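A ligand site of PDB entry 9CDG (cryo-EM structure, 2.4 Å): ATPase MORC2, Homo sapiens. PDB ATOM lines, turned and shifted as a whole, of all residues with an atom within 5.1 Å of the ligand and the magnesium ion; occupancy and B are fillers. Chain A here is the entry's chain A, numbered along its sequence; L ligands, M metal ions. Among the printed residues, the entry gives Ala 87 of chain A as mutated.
The backbone NH of Leu 104 lies within hydrogen-bond range of an oxygen (O7) of the ligand, 3.4 Å away. N3 of the ligand is in hydrogen-bond range of OD2 of Asp 68, at 3.2 Å. The backbone NH (N) of Gly 101 lies within hydrogen-bond range of an oxygen (O4) of the ligand. An oxygen (O3) of the ligand lies within salt-bridge range of the side-chain amino group (NZ) of Lys 427, 3.0 Å away. An oxygen (O7) of the ligand lies within hydrogen-bond range of the backbone NH of Asn 102 (3.0 Å). An oxygen (O1) of the ligand is in hydrogen-bond range of the backbone NH of Gly 103 (2.8 Å). An oxygen (O8) of the ligand lies close to the side-chain amide oxygen of Asn 39 (2.9 Å). A nitrogen (N4) of the ligand lies within hydrogen-bond range of the side-chain hydroxyl (OG1) of Thr 197 (3.4 Å). The backbone NH of Tyr 100 is in hydrogen-bond range of an oxygen (O3) of the ligand (2.4 Å). The backbone NH (N) of Gln 99 sits at hydrogen-bond distance from an oxygen (O3) of the ligand (2.6 Å). An oxygen (O7) of the ligand is in salt-bridge range of the side-chain amino group of Lys 105, 2.8 Å away.
The backbone NH (N) of Gly 98 is in hydrogen-bond range of the side-chain carboxylate (OD2) of Asp 42, at 2.8 Å. The side-chain amide oxygen of Gln 99 lies close to the backbone carbonyl oxygen of Ile 97, 3.0 Å away. NZ of Lys 427 sits at hydrogen-bond distance from O of Ile 97 (3.2 Å). The side-chain amino group of Lys 105 sits at hydrogen-bond distance from the backbone carbonyl oxygen of Gly 101. OE2 of Glu 35 is in salt-bridge range of NZ of Lys 427 (3.2 Å). The side-chain amide nitrogen (ND2) of Asn 39 lies within hydrogen-bond range of the backbone carbonyl oxygen (O) of Glu 35 (3.0 Å). The backbone NH of Asp 68 is in hydrogen-bond range of the backbone carbonyl oxygen of Thr 197, at 2.9 Å. NZ of Lys 105 is in hydrogen-bond range of O of Val 81 (2.7 Å).
An oxygen (O2) of the ligand sits close to the side-chain carboxylate of Glu 35 (2.9 Å). N5 of the ligand sits close to SD of Met 73 (3.2 Å). Ala 43 touches the ligand (CB to N4, 3.4 Å). CG2 of Val 81 touches O11 of the ligand (3.3 Å). CA of Gly 98 touches O3 of the ligand (3.3 Å). Hydrophobic or aromatic side chains that line the ligand: Ala 43, Met 73, Val 81, Tyr 100 and Leu 104. Of the 25 residues printed, 16 come within 4 Å of the ligand. The nearest printed residue that does not touch the ligand is Asp 42 (4.1 Å).
Residues that only touch the magnesium ion: Glu 35 (3.2 Å), Gly 103 (3.5 Å) and Leu 104 (3.9 Å). Of the 25 residues printed, 4 come within 4 Å of the magnesium ion. Along chain A the residues within 4 Å of the magnesium ion span positions 35 to 104.
The magnesium ion is bound by O8 of the ligand, O5 of the ligand, O2 of the ligand and O6 of the ligand. Slightly farther from the magnesium ion lies O9 of the ligand (2.7 Å). Slightly farther from the magnesium ion lies OD1 of Asn 39 (2.8 Å).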
ATOM      1  N   GLU A  35      -6.583 -35.415  28.866  1.00  0.00           N
ATOM      2  CA  GLU A  35      -6.015 -34.071  28.869  1.00  0.00           C
ATOM      3  C   GLU A  35      -5.866 -33.504  27.456  1.00  0.00           C
ATOM      4  O   GLU A  35      -6.122 -32.321  27.229  1.00  0.00           O
ATOM      5  CB  GLU A  35      -4.674 -34.065  29.596  1.00  0.00           C
ATOM      6  CG  GLU A  35      -4.758 -33.413  30.974  1.00  0.00           C
ATOM      7  CD  GLU A  35      -5.297 -31.989  30.923  1.00  0.00           C
ATOM      8  OE1 GLU A  35      -4.966 -31.220  29.981  1.00  0.00           O
ATOM      9  OE2 GLU A  35      -6.068 -31.626  31.824  1.00  0.00           O
ATOM     10  N   ASN A  39      -7.737 -30.241  25.879  1.00  0.00           N
ATOM     11  CA  ASN A  39      -7.121 -29.142  25.130  1.00  0.00           C
ATOM     12  C   ASN A  39      -7.820 -28.925  23.801  1.00  0.00           C
ATOM     13  O   ASN A  39      -7.991 -27.783  23.352  1.00  0.00           O
ATOM     14  CB  ASN A  39      -5.640 -29.416  24.932  1.00  0.00           C
ATOM     15  CG  ASN A  39      -4.923 -29.656  26.229  1.00  0.00           C
ATOM     16  OD1 ASN A  39      -5.245 -29.056  27.252  1.00  0.00           O
ATOM     17  ND2 ASN A  39      -3.950 -30.554  26.203  1.00  0.00           N
ATOM     18  N   ALA A  40      -8.262 -30.022  23.172  1.00  0.00           N
ATOM     19  CA  ALA A  40      -9.057 -29.868  21.958  1.00  0.00           C
ATOM     20  C   ALA A  40     -10.433 -29.266  22.246  1.00  0.00           C
ATOM     21  O   ALA A  40     -10.991 -28.585  21.380  1.00  0.00           O
ATOM     22  CB  ALA A  40      -9.199 -31.217  21.261  1.00  0.00           C
ATOM     23  N   ASP A  42     -10.907 -27.026  24.677  1.00  0.00           N
ATOM     24  CA  ASP A  42     -10.539 -25.625  24.860  1.00  0.00           C
ATOM     25  C   ASP A  42     -10.225 -24.934  23.542  1.00  0.00           C
ATOM     26  O   ASP A  42     -10.277 -23.700  23.486  1.00  0.00           O
ATOM     27  CB  ASP A  42      -9.336 -25.532  25.793  1.00  0.00           C
ATOM     28  CG  ASP A  42      -9.606 -26.115  27.152  1.00  0.00           C
ATOM     29  OD1 ASP A  42     -10.791 -26.330  27.483  1.00  0.00           O
ATOM     30  OD2 ASP A  42      -8.632 -26.367  27.888  1.00  0.00           O
ATOM     31  N   ALA A  43      -9.913 -25.694  22.503  1.00  0.00           N
ATOM     32  CA  ALA A  43      -9.723 -25.158  21.162  1.00  0.00           C
ATOM     33  C   ALA A  43     -11.018 -24.766  20.457  1.00  0.00           C
ATOM     34  O   ALA A  43     -10.947 -24.250  19.335  1.00  0.00           O
ATOM     35  CB  ALA A  43      -9.001 -26.182  20.294  1.00  0.00           C
ATOM     36  N   ASP A  68      -7.786 -32.491  15.742  1.00  0.00           N
ATOM     37  CA  ASP A  68      -8.982 -31.721  16.020  1.00  0.00           C
ATOM     38  C   ASP A  68      -9.023 -30.505  15.103  1.00  0.00           C
ATOM     39  O   ASP A  68      -7.990 -30.047  14.599  1.00  0.00           O
ATOM     40  CB  ASP A  68      -9.059 -31.280  17.478  1.00  0.00           C
ATOM     41  CG  ASP A  68      -7.892 -30.410  17.892  1.00  0.00           C
ATOM     42  OD1 ASP A  68      -8.002 -29.174  17.766  1.00  0.00           O
ATOM     43  OD2 ASP A  68      -6.880 -30.964  18.343  1.00  0.00           O
ATOM     44  N   GLY A  72      -6.437 -23.909  16.820  1.00  0.00           N
ATOM     45  CA  GLY A  72      -5.043 -24.044  16.468  1.00  0.00           C
ATOM     46  C   GLY A  72      -4.166 -23.094  17.270  1.00  0.00           C
ATOM     47  O   GLY A  72      -4.594 -22.467  18.233  1.00  0.00           O
ATOM     48  N   MET A  73      -2.917 -22.994  16.843  1.00  0.00           N
ATOM     49  CA  MET A  73      -1.945 -22.144  17.522  1.00  0.00           C
ATOM     50  C   MET A  73      -1.217 -21.265  16.516  1.00  0.00           C
ATOM     51  O   MET A  73      -0.915 -21.693  15.406  1.00  0.00           O
ATOM     52  CB  MET A  73      -0.919 -22.962  18.285  1.00  0.00           C
ATOM     53  CG  MET A  73      -1.177 -23.085  19.759  1.00  0.00           C
ATOM     54  SD  MET A  73      -2.099 -24.571  20.066  1.00  0.00           S
ATOM     55  CE  MET A  73      -0.784 -25.780  20.127  1.00  0.00           C
ATOM     56  N   SER A  80       4.093 -20.634  23.882  1.00  0.00           N
ATOM     57  CA  SER A  80       3.534 -20.666  25.220  1.00  0.00           C
ATOM     58  C   SER A  80       3.057 -22.054  25.626  1.00  0.00           C
ATOM     59  O   SER A  80       2.669 -22.238  26.788  1.00  0.00           O
ATOM     60  CB  SER A  80       2.370 -19.687  25.329  1.00  0.00           C
ATOM     61  OG  SER A  80       1.127 -20.359  25.221  1.00  0.00           O
ATOM     62  N   VAL A  81       3.032 -23.018  24.702  1.00  0.00           N
ATOM     63  CA  VAL A  81       2.736 -24.401  25.068  1.00  0.00           C
ATOM     64  C   VAL A  81       3.820 -24.951  25.996  1.00  0.00           C
ATOM     65  O   VAL A  81       3.532 -25.518  27.052  1.00  0.00           O
ATOM     66  CB  VAL A  81       2.587 -25.272  23.808  1.00  0.00           C
ATOM     67  CG1 VAL A  81       2.677 -26.747  24.152  1.00  0.00           C
ATOM     68  CG2 VAL A  81       1.283 -24.971  23.123  1.00  0.00           C
ATOM     69  N   LYS A  86       0.170 -21.780  32.288  1.00  0.00           N
ATOM     70  CA  LYS A  86      -0.276 -20.668  31.457  1.00  0.00           C
ATOM     71  C   LYS A  86      -1.726 -20.353  31.797  1.00  0.00           C
ATOM     72  O   LYS A  86      -2.319 -20.942  32.708  1.00  0.00           O
ATOM     73  CB  LYS A  86      -0.103 -20.992  29.966  1.00  0.00           C
ATOM     74  CG  LYS A  86       1.308 -20.768  29.428  1.00  0.00           C
ATOM     75  CD  LYS A  86       1.783 -19.350  29.691  1.00  0.00           C
ATOM     76  CE  LYS A  86       1.092 -18.369  28.771  1.00  0.00           C
ATOM     77  NZ  LYS A  86       1.384 -16.960  29.162  1.00  0.00           N
ATOM     78  N   ALA A  87      -2.291 -19.407  31.032  1.00  0.00           N
ATOM     79  CA  ALA A  87      -3.664 -18.895  31.159  1.00  0.00           C
ATOM     80  C   ALA A  87      -3.981 -18.390  32.567  1.00  0.00           C
ATOM     81  O   ALA A  87      -3.733 -17.224  32.880  1.00  0.00           O
ATOM     82  CB  ALA A  87      -4.681 -19.967  30.732  1.00  0.00           C
ATOM     83  N   ILE A  97     -11.509 -25.536  30.369  1.00  0.00           N
ATOM     84  CA  ILE A  97     -11.013 -26.575  31.272  1.00  0.00           C
ATOM     85  C   ILE A  97      -9.557 -26.349  31.613  1.00  0.00           C
ATOM     86  O   ILE A  97      -9.148 -26.476  32.771  1.00  0.00           O
ATOM     87  CB  ILE A  97     -11.237 -27.959  30.633  1.00  0.00           C
ATOM     88  CG1 ILE A  97     -12.722 -28.145  30.333  1.00  0.00           C
ATOM     89  CG2 ILE A  97     -10.751 -29.062  31.546  1.00  0.00           C
ATOM     90  CD1 ILE A  97     -13.003 -29.348  29.507  1.00  0.00           C
ATOM     91  N   GLY A  98      -8.748 -25.981  30.619  1.00  0.00           N
ATOM     92  CA  GLY A  98      -7.330 -25.815  30.827  1.00  0.00           C
ATOM     93  C   GLY A  98      -6.937 -24.562  31.569  1.00  0.00           C
ATOM     94  O   GLY A  98      -7.123 -23.446  31.078  1.00  0.00           O
ATOM     95  N   GLN A  99      -6.389 -24.725  32.779  1.00  0.00           N
ATOM     96  CA  GLN A  99      -5.867 -23.612  33.541  1.00  0.00           C
ATOM     97  C   GLN A  99      -4.501 -23.882  34.154  1.00  0.00           C
ATOM     98  O   GLN A  99      -3.840 -22.922  34.587  1.00  0.00           O
ATOM     99  CB  GLN A  99      -6.846 -23.212  34.652  1.00  0.00           C
ATOM    100  CG  GLN A  99      -6.659 -23.943  35.970  1.00  0.00           C
ATOM    101  CD  GLN A  99      -7.510 -25.196  36.088  1.00  0.00           C
ATOM    102  OE1 GLN A  99      -7.477 -26.053  35.201  1.00  0.00           O
ATOM    103  NE2 GLN A  99      -8.256 -25.302  37.171  1.00  0.00           N
ATOM    104  N   TYR A 100      -4.049 -25.126  34.191  1.00  0.00           N
ATOM    105  CA  TYR A 100      -2.780 -25.446  34.840  1.00  0.00           C
ATOM    106  C   TYR A 100      -1.586 -25.295  33.925  1.00  0.00           C
ATOM    107  O   TYR A 100      -0.457 -25.279  34.413  1.00  0.00           O
ATOM    108  CB  TYR A 100      -2.824 -26.871  35.387  1.00  0.00           C
ATOM    109  CG  TYR A 100      -3.668 -27.015  36.622  1.00  0.00           C
ATOM    110  CD1 TYR A 100      -3.905 -25.938  37.457  1.00  0.00           C
ATOM    111  CD2 TYR A 100      -4.225 -28.232  36.960  1.00  0.00           C
ATOM    112  CE1 TYR A 100      -4.676 -26.068  38.588  1.00  0.00           C
ATOM    113  CE2 TYR A 100      -4.999 -28.378  38.086  1.00  0.00           C
ATOM    114  CZ  TYR A 100      -5.223 -27.287  38.891  1.00  0.00           C
ATOM    115  OH  TYR A 100      -5.990 -27.441  40.016  1.00  0.00           O
ATOM    116  N   GLY A 101      -1.799 -25.189  32.610  1.00  0.00           N
ATOM    117  CA  GLY A 101      -0.718 -25.047  31.669  1.00  0.00           C
ATOM    118  C   GLY A 101       0.195 -26.244  31.575  1.00  0.00           C
ATOM    119  O   GLY A 101       1.369 -26.093  31.201  1.00  0.00           O
ATOM    120  N   ASN A 102      -0.289 -27.434  31.903  1.00  0.00           N
ATOM    121  CA  ASN A 102       0.590 -28.572  32.120  1.00  0.00           C
ATOM    122  C   ASN A 102       0.126 -29.837  31.416  1.00  0.00           C
ATOM    123  O   ASN A 102       0.942 -30.698  31.059  1.00  0.00           O
ATOM    124  CB  ASN A 102       0.684 -28.846  33.620  1.00  0.00           C
ATOM    125  CG  ASN A 102       1.681 -29.916  33.941  1.00  0.00           C
ATOM    126  OD1 ASN A 102       1.420 -30.797  34.751  1.00  0.00           O
ATOM    127  ND2 ASN A 102       2.832 -29.851  33.295  1.00  0.00           N
ATOM    128  N   GLY A 103      -1.190 -29.934  31.187  1.00  0.00           N
ATOM    129  CA  GLY A 103      -1.844 -31.205  30.929  1.00  0.00           C
ATOM    130  C   GLY A 103      -1.426 -31.917  29.667  1.00  0.00           C
ATOM    131  O   GLY A 103      -1.329 -33.150  29.676  1.00  0.00           O
ATOM    132  N   LEU A 104      -1.167 -31.172  28.592  1.00  0.00           N
ATOM    133  CA  LEU A 104      -0.661 -31.791  27.372  1.00  0.00           C
ATOM    134  C   LEU A 104       0.722 -32.394  27.595  1.00  0.00           C
ATOM    135  O   LEU A 104       0.994 -33.526  27.179  1.00  0.00           O
ATOM    136  CB  LEU A 104      -0.619 -30.769  26.243  1.00  0.00           C
ATOM    137  CG  LEU A 104       0.332 -31.002  25.072  1.00  0.00           C
ATOM    138  CD1 LEU A 104      -0.182 -32.121  24.189  1.00  0.00           C
ATOM    139  CD2 LEU A 104       0.480 -29.737  24.275  1.00  0.00           C
ATOM    140  N   LYS A 105       1.592 -31.666  28.289  1.00  0.00           N
ATOM    141  CA  LYS A 105       2.950 -32.129  28.535  1.00  0.00           C
ATOM    142  C   LYS A 105       2.969 -33.311  29.493  1.00  0.00           C
ATOM    143  O   LYS A 105       3.812 -34.205  29.356  1.00  0.00           O
ATOM    144  CB  LYS A 105       3.801 -30.981  29.080  1.00  0.00           C
ATOM    145  CG  LYS A 105       4.275 -30.009  28.021  1.00  0.00           C
ATOM    146  CD  LYS A 105       3.327 -28.826  27.859  1.00  0.00           C
ATOM    147  CE  LYS A 105       3.133 -28.083  29.169  1.00  0.00           C
ATOM    148  NZ  LYS A 105       2.269 -26.891  28.987  1.00  0.00           N
ATOM    149  N   LEU A 117       3.753 -32.298  17.581  1.00  0.00           N
ATOM    150  CA  LEU A 117       2.490 -31.586  17.505  1.00  0.00           C
ATOM    151  C   LEU A 117       2.481 -30.704  16.270  1.00  0.00           C
ATOM    152  O   LEU A 117       3.383 -29.880  16.096  1.00  0.00           O
ATOM    153  CB  LEU A 117       2.279 -30.734  18.757  1.00  0.00           C
ATOM    154  CG  LEU A 117       1.016 -29.903  18.919  1.00  0.00           C
ATOM    155  CD1 LEU A 117       0.471 -30.072  20.315  1.00  0.00           C
ATOM    156  CD2 LEU A 117       1.317 -28.448  18.672  1.00  0.00           C
ATOM    157  N   THR A 197      -5.387 -28.596  15.050  1.00  0.00           N
ATOM    158  CA  THR A 197      -4.199 -29.100  15.724  1.00  0.00           C
ATOM    159  C   THR A 197      -4.161 -30.617  15.616  1.00  0.00           C
ATOM    160  O   THR A 197      -5.144 -31.287  15.947  1.00  0.00           O
ATOM    161  CB  THR A 197      -4.176 -28.676  17.198  1.00  0.00           C
ATOM    162  OG1 THR A 197      -4.282 -27.249  17.278  1.00  0.00           O
ATOM    163  CG2 THR A 197      -2.896 -29.122  17.868  1.00  0.00           C
ATOM    164  N   VAL A 199      -1.968 -33.678  17.148  1.00  0.00           N
ATOM    165  CA  VAL A 199      -1.003 -34.079  18.160  1.00  0.00           C
ATOM    166  C   VAL A 199      -0.715 -35.555  17.958  1.00  0.00           C
ATOM    167  O   VAL A 199      -1.625 -36.385  18.060  1.00  0.00           O
ATOM    168  CB  VAL A 199      -1.506 -33.801  19.575  1.00  0.00           C
ATOM    169  CG1 VAL A 199      -0.332 -33.750  20.519  1.00  0.00           C
ATOM    170  CG2 VAL A 199      -2.282 -32.504  19.629  1.00  0.00           C
ATOM    171  N   LYS A 427      -5.800 -34.107  37.061  1.00  0.00           N
ATOM    172  CA  LYS A 427      -7.238 -33.843  36.942  1.00  0.00           C
ATOM    173  C   LYS A 427      -8.056 -35.121  37.100  1.00  0.00           C
ATOM    174  O   LYS A 427      -9.020 -35.363  36.384  1.00  0.00           O
ATOM    175  CB  LYS A 427      -7.572 -33.125  35.632  1.00  0.00           C
ATOM    176  CG  LYS A 427      -6.779 -31.856  35.420  1.00  0.00           C
ATOM    177  CD  LYS A 427      -7.569 -30.819  34.647  1.00  0.00           C
ATOM    178  CE  LYS A 427      -6.727 -29.586  34.385  1.00  0.00           C
ATOM    179  NZ  LYS A 427      -7.159 -28.892  33.147  1.00  0.00           N
HETATM  180  P1  LIG L   1      -4.244 -27.824  31.849  1.00  0.00           P
HETATM  181  O1  LIG L   1      -3.329 -28.771  32.523  1.00  0.00           O
HETATM  182  O2  LIG L   1      -5.244 -28.478  30.904  1.00  0.00           O
HETATM  183  O3  LIG L   1      -4.989 -26.919  32.814  1.00  0.00           O
HETATM  184  P2  LIG L   1      -3.606 -25.962  29.606  1.00  0.00           P
HETATM  185  O4  LIG L   1      -3.819 -24.541  29.897  1.00  0.00           O
HETATM  186  O5  LIG L   1      -4.669 -26.634  28.752  1.00  0.00           O
HETATM  187  O6  LIG L   1      -3.427 -26.823  30.932  1.00  0.00           O
HETATM  188  P3  LIG L   1      -1.462 -27.391  28.161  1.00  0.00           P
HETATM  189  O7  LIG L   1      -0.327 -27.919  28.935  1.00  0.00           O
HETATM  190  O8  LIG L   1      -2.515 -28.429  27.802  1.00  0.00           O
HETATM  191  O9  LIG L   1      -2.205 -26.209  28.891  1.00  0.00           O
HETATM  192  O10 LIG L   1      -0.963 -26.665  26.859  1.00  0.00           O
HETATM  193  C1  LIG L   1      -0.572 -25.282  26.876  1.00  0.00           C
HETATM  194  C2  LIG L   1      -1.412 -24.573  25.855  1.00  0.00           C
HETATM  195  O11 LIG L   1      -1.569 -25.439  24.716  1.00  0.00           O
HETATM  196  C3  LIG L   1      -2.823 -24.210  26.310  1.00  0.00           C
HETATM  197  O12 LIG L   1      -2.944 -22.813  26.567  1.00  0.00           O
HETATM  198  C4  LIG L   1      -3.737 -24.645  25.153  1.00  0.00           C
HETATM  199  O13 LIG L   1      -4.527 -23.557  24.682  1.00  0.00           O
HETATM  200  C5  LIG L   1      -2.768 -25.096  24.071  1.00  0.00           C
HETATM  201  N1  LIG L   1      -3.199 -26.275  23.331  1.00  0.00           N
HETATM  202  C6  LIG L   1      -2.797 -27.569  23.531  1.00  0.00           C
HETATM  203  N2  LIG L   1      -3.358 -28.431  22.720  1.00  0.00           N
HETATM  204  C7  LIG L   1      -4.179 -27.654  21.935  1.00  0.00           C
HETATM  205  C8  LIG L   1      -5.054 -27.960  20.869  1.00  0.00           C
HETATM  206  N3  LIG L   1      -5.243 -29.204  20.407  1.00  0.00           N
HETATM  207  N4  LIG L   1      -5.733 -26.945  20.296  1.00  0.00           N
HETATM  208  C9  LIG L   1      -5.538 -25.707  20.757  1.00  0.00           C
HETATM  209  N5  LIG L   1      -4.763 -25.289  21.757  1.00  0.00           N
HETATM  210  C10 LIG L   1      -4.103 -26.321  22.298  1.00  0.00           C
HETATM  211 MG    MG M   1      -3.746 -28.352  29.460  1.00  0.00          MG
